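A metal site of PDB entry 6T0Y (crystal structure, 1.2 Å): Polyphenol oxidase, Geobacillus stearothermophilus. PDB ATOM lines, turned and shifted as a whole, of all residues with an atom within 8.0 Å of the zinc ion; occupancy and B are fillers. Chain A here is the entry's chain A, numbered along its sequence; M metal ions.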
ATOM      1  N   ALA A 179     -25.545 -34.196  -9.305  1.00  0.00           N
ATOM      2  CA  ALA A 179     -25.860 -33.635  -8.000  1.00  0.00           C
ATOM      3  C   ALA A 179     -25.850 -32.127  -8.175  1.00  0.00           C
ATOM      4  O   ALA A 179     -25.484 -31.608  -9.233  1.00  0.00           O
ATOM      5  CB  ALA A 179     -24.840 -34.103  -6.964  1.00  0.00           C
ATOM      6  N   ILE A 180     -26.257 -31.412  -7.139  1.00  0.00           N
ATOM      7  CA  ILE A 180     -26.291 -29.964  -7.264  1.00  0.00           C
ATOM      8  C   ILE A 180     -24.871 -29.424  -7.246  1.00  0.00           C
ATOM      9  O   ILE A 180     -24.037 -29.842  -6.451  1.00  0.00           O
ATOM     10  CB  ILE A 180     -27.192 -29.340  -6.187  1.00  0.00           C
ATOM     11  CG1 ILE A 180     -27.442 -27.854  -6.518  1.00  0.00           C
ATOM     12  CG2 ILE A 180     -26.610 -29.526  -4.808  1.00  0.00           C
ATOM     13  CD1 ILE A 180     -28.543 -27.239  -5.746  1.00  0.00           C
ATOM     14  N   GLY A 181     -24.589 -28.520  -8.163  1.00  0.00           N
ATOM     15  CA  GLY A 181     -23.269 -27.945  -8.301  1.00  0.00           C
ATOM     16  C   GLY A 181     -23.109 -26.626  -7.573  1.00  0.00           C
ATOM     17  O   GLY A 181     -24.077 -26.047  -7.071  1.00  0.00           O
ATOM     18  N   PRO A 182     -21.868 -26.136  -7.495  1.00  0.00           N
ATOM     19  CA  PRO A 182     -21.625 -24.849  -6.811  1.00  0.00           C
ATOM     20  C   PRO A 182     -22.219 -23.689  -7.556  1.00  0.00           C
ATOM     21  O   PRO A 182     -22.367 -22.609  -6.981  1.00  0.00           O
ATOM     22  CB  PRO A 182     -20.089 -24.767  -6.750  1.00  0.00           C
ATOM     23  CG  PRO A 182     -19.609 -25.609  -7.890  1.00  0.00           C
ATOM     24  CD  PRO A 182     -20.630 -26.726  -8.029  1.00  0.00           C
ATOM     25  N   CYS A 183     -22.550 -23.891  -8.829  1.00  0.00           N
ATOM     26  CA  CYS A 183     -23.336 -22.939  -9.608  1.00  0.00           C
ATOM     27  C   CYS A 183     -24.654 -22.609  -8.931  1.00  0.00           C
ATOM     28  O   CYS A 183     -25.157 -21.483  -9.066  1.00  0.00           O
ATOM     29  CB  CYS A 183     -23.593 -23.561 -10.989  1.00  0.00           C
ATOM     30  SG  CYS A 183     -24.014 -25.365 -10.962  1.00  0.00           S
ATOM     31  N   CYS A 184     -25.223 -23.557  -8.187  1.00  0.00           N
ATOM     32  CA  CYS A 184     -26.573 -23.452  -7.667  1.00  0.00           C
ATOM     33  C   CYS A 184     -26.682 -23.636  -6.159  1.00  0.00           C
ATOM     34  O   CYS A 184     -27.740 -23.312  -5.604  1.00  0.00           O
ATOM     35  CB  CYS A 184     -27.491 -24.486  -8.347  1.00  0.00           C
ATOM     36  SG  CYS A 184     -27.690 -24.258 -10.146  1.00  0.00           S
ATOM     37  N   TYR A 185     -25.666 -24.154  -5.481  1.00  0.00           N
ATOM     38  CA  TYR A 185     -25.763 -24.510  -4.068  1.00  0.00           C
ATOM     39  C   TYR A 185     -24.932 -23.533  -3.244  1.00  0.00           C
ATOM     40  O   TYR A 185     -23.692 -23.573  -3.276  1.00  0.00           O
ATOM     41  CB  TYR A 185     -25.288 -25.944  -3.841  1.00  0.00           C
ATOM     42  CG  TYR A 185     -25.591 -26.529  -2.499  1.00  0.00           C
ATOM     43  CD1 TYR A 185     -26.704 -26.149  -1.784  1.00  0.00           C
ATOM     44  CD2 TYR A 185     -24.775 -27.497  -1.953  1.00  0.00           C
ATOM     45  CE1 TYR A 185     -26.987 -26.714  -0.546  1.00  0.00           C
ATOM     46  CE2 TYR A 185     -25.055 -28.077  -0.724  1.00  0.00           C
ATOM     47  CZ  TYR A 185     -26.159 -27.681  -0.022  1.00  0.00           C
ATOM     48  OH  TYR A 185     -26.376 -28.273   1.213  1.00  0.00           O
ATOM     49  N   GLU A 241     -20.200 -34.019 -14.419  1.00  0.00           N
ATOM     50  CA  GLU A 241     -20.322 -32.569 -14.406  1.00  0.00           C
ATOM     51  C   GLU A 241     -21.769 -32.106 -14.456  1.00  0.00           C
ATOM     52  O   GLU A 241     -22.024 -30.900 -14.488  1.00  0.00           O
ATOM     53  CB  GLU A 241     -19.523 -31.979 -15.569  1.00  0.00           C
ATOM     54  CG  GLU A 241     -17.998 -32.139 -15.363  1.00  0.00           C
ATOM     55  CD  GLU A 241     -17.191 -32.062 -16.649  1.00  0.00           C
ATOM     56  OE1 GLU A 241     -16.115 -32.697 -16.702  1.00  0.00           O
ATOM     57  OE2 GLU A 241     -17.637 -31.390 -17.592  1.00  0.00           O
ATOM     58  N   ARG A 242     -22.727 -33.027 -14.437  1.00  0.00           N
ATOM     59  CA  ARG A 242     -24.124 -32.655 -14.514  1.00  0.00           C
ATOM     60  C   ARG A 242     -24.618 -32.125 -13.171  1.00  0.00           C
ATOM     61  O   ARG A 242     -24.419 -32.767 -12.139  1.00  0.00           O
ATOM     62  CB  ARG A 242     -24.968 -33.854 -14.912  1.00  0.00           C
ATOM     63  CG  ARG A 242     -24.621 -34.460 -16.245  1.00  0.00           C
ATOM     64  CD  ARG A 242     -25.440 -35.681 -16.532  1.00  0.00           C
ATOM     65  NE  ARG A 242     -25.174 -36.326 -17.814  1.00  0.00           N
ATOM     66  CZ  ARG A 242     -25.779 -36.034 -18.960  1.00  0.00           C
ATOM     67  NH1 ARG A 242     -26.697 -35.086 -19.011  1.00  0.00           N
ATOM     68  NH2 ARG A 242     -25.482 -36.737 -20.027  1.00  0.00           N
ATOM     69  N   CYS A 243     -25.282 -30.962 -13.214  1.00  0.00           N
ATOM     70  CA  CYS A 243     -25.940 -30.343 -12.077  1.00  0.00           C
ATOM     71  C   CYS A 243     -27.439 -30.600 -12.155  1.00  0.00           C
ATOM     72  O   CYS A 243     -28.078 -30.292 -13.158  1.00  0.00           O
ATOM     73  CB  CYS A 243     -25.675 -28.827 -12.063  1.00  0.00           C
ATOM     74  SG  CYS A 243     -26.600 -27.918 -10.799  1.00  0.00           S
ATOM     75  N   THR A 244     -28.002 -31.140 -11.067  1.00  0.00           N
ATOM     76  CA  THR A 244     -29.418 -31.477 -11.034  1.00  0.00           C
ATOM     77  C   THR A 244     -30.306 -30.243 -11.085  1.00  0.00           C
ATOM     78  O   THR A 244     -31.410 -30.295 -11.621  1.00  0.00           O
ATOM     79  CB  THR A 244     -29.719 -32.273  -9.773  1.00  0.00           C
ATOM     80  OG1 THR A 244     -29.113 -31.634  -8.646  1.00  0.00           O
ATOM     81  CG2 THR A 244     -29.191 -33.658  -9.879  1.00  0.00           C
ATOM     82  N   SER A 245     -29.842 -29.125 -10.526  1.00  0.00           N
ATOM     83  CA  SER A 245     -30.629 -27.895 -10.596  1.00  0.00           C
ATOM     84  C   SER A 245     -30.562 -27.274 -11.991  1.00  0.00           C
ATOM     85  O   SER A 245     -31.593 -26.868 -12.536  1.00  0.00           O
ATOM     86  CB  SER A 245     -30.131 -26.923  -9.541  1.00  0.00           C
ATOM     87  OG  SER A 245     -30.638 -25.639  -9.801  1.00  0.00           O
ATOM     88  N   CYS A 246     -29.378 -27.223 -12.592  1.00  0.00           N
ATOM     89  CA  CYS A 246     -29.242 -26.645 -13.929  1.00  0.00           C
ATOM     90  C   CYS A 246     -29.973 -27.459 -14.999  1.00  0.00           C
ATOM     91  O   CYS A 246     -30.563 -26.876 -15.921  1.00  0.00           O
ATOM     92  CB  CYS A 246     -27.764 -26.538 -14.329  1.00  0.00           C
ATOM     93  SG  CYS A 246     -26.821 -25.253 -13.504  1.00  0.00           S
ATOM     94  N   GLU A 247     -29.891 -28.783 -14.950  1.00  0.00           N
ATOM     95  CA  GLU A 247     -30.388 -29.653 -16.024  1.00  0.00           C
ATOM     96  C   GLU A 247     -31.838 -30.024 -15.723  1.00  0.00           C
ATOM     97  O   GLU A 247     -32.196 -31.179 -15.481  1.00  0.00           O
ATOM     98  CB  GLU A 247     -29.466 -30.859 -16.211  1.00  0.00           C
ATOM     99  CG  GLU A 247     -28.038 -30.424 -16.557  1.00  0.00           C
ATOM    100  CD  GLU A 247     -27.076 -31.508 -17.020  1.00  0.00           C
ATOM    101  OE1 GLU A 247     -27.481 -32.657 -17.320  1.00  0.00           O
ATOM    102  OE2 GLU A 247     -25.864 -31.200 -17.104  1.00  0.00           O
ATOM    103  N   SER A 253     -35.030 -31.493  -8.705  1.00  0.00           N
ATOM    104  CA  SER A 253     -34.072 -30.795  -7.845  1.00  0.00           C
ATOM    105  C   SER A 253     -34.796 -30.233  -6.637  1.00  0.00           C
ATOM    106  O   SER A 253     -35.668 -29.360  -6.786  1.00  0.00           O
ATOM    107  CB  SER A 253     -33.393 -29.659  -8.617  1.00  0.00           C
ATOM    108  OG  SER A 253     -32.665 -28.801  -7.743  1.00  0.00           O
HETATM  109 ZN    ZN M   1     -26.282 -25.692 -11.311  1.00  0.00          ZN
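SG of Cys 243 sits close to N of Ser 245 (3.5 Å). The backbone NH of Gly 181 sits close to the side-chain sulfur of Cys 243 (3.4 Å). The side-chain sulfur of Cys 184 sits close to the side-chain hydroxyl of Ser 245 (3.3 Å).
Four residues have an atom within 4 Å of the zinc ion: Cys 183, Cys 184, Cys 243 and Cys 246. The nearest printed residue that does not touch the zinc ion is Ser 245 (4.4 Å).
The zinc ion is bound by SG of Cys 246. The zinc ion is bound by the side-chain sulfur (SG) of Cys 243, 2.3 Å away. SG of Cys 183 binds the zinc ion, 2.3 Å away. SG of Cys 184 binds the zinc ion (2.3 Å).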
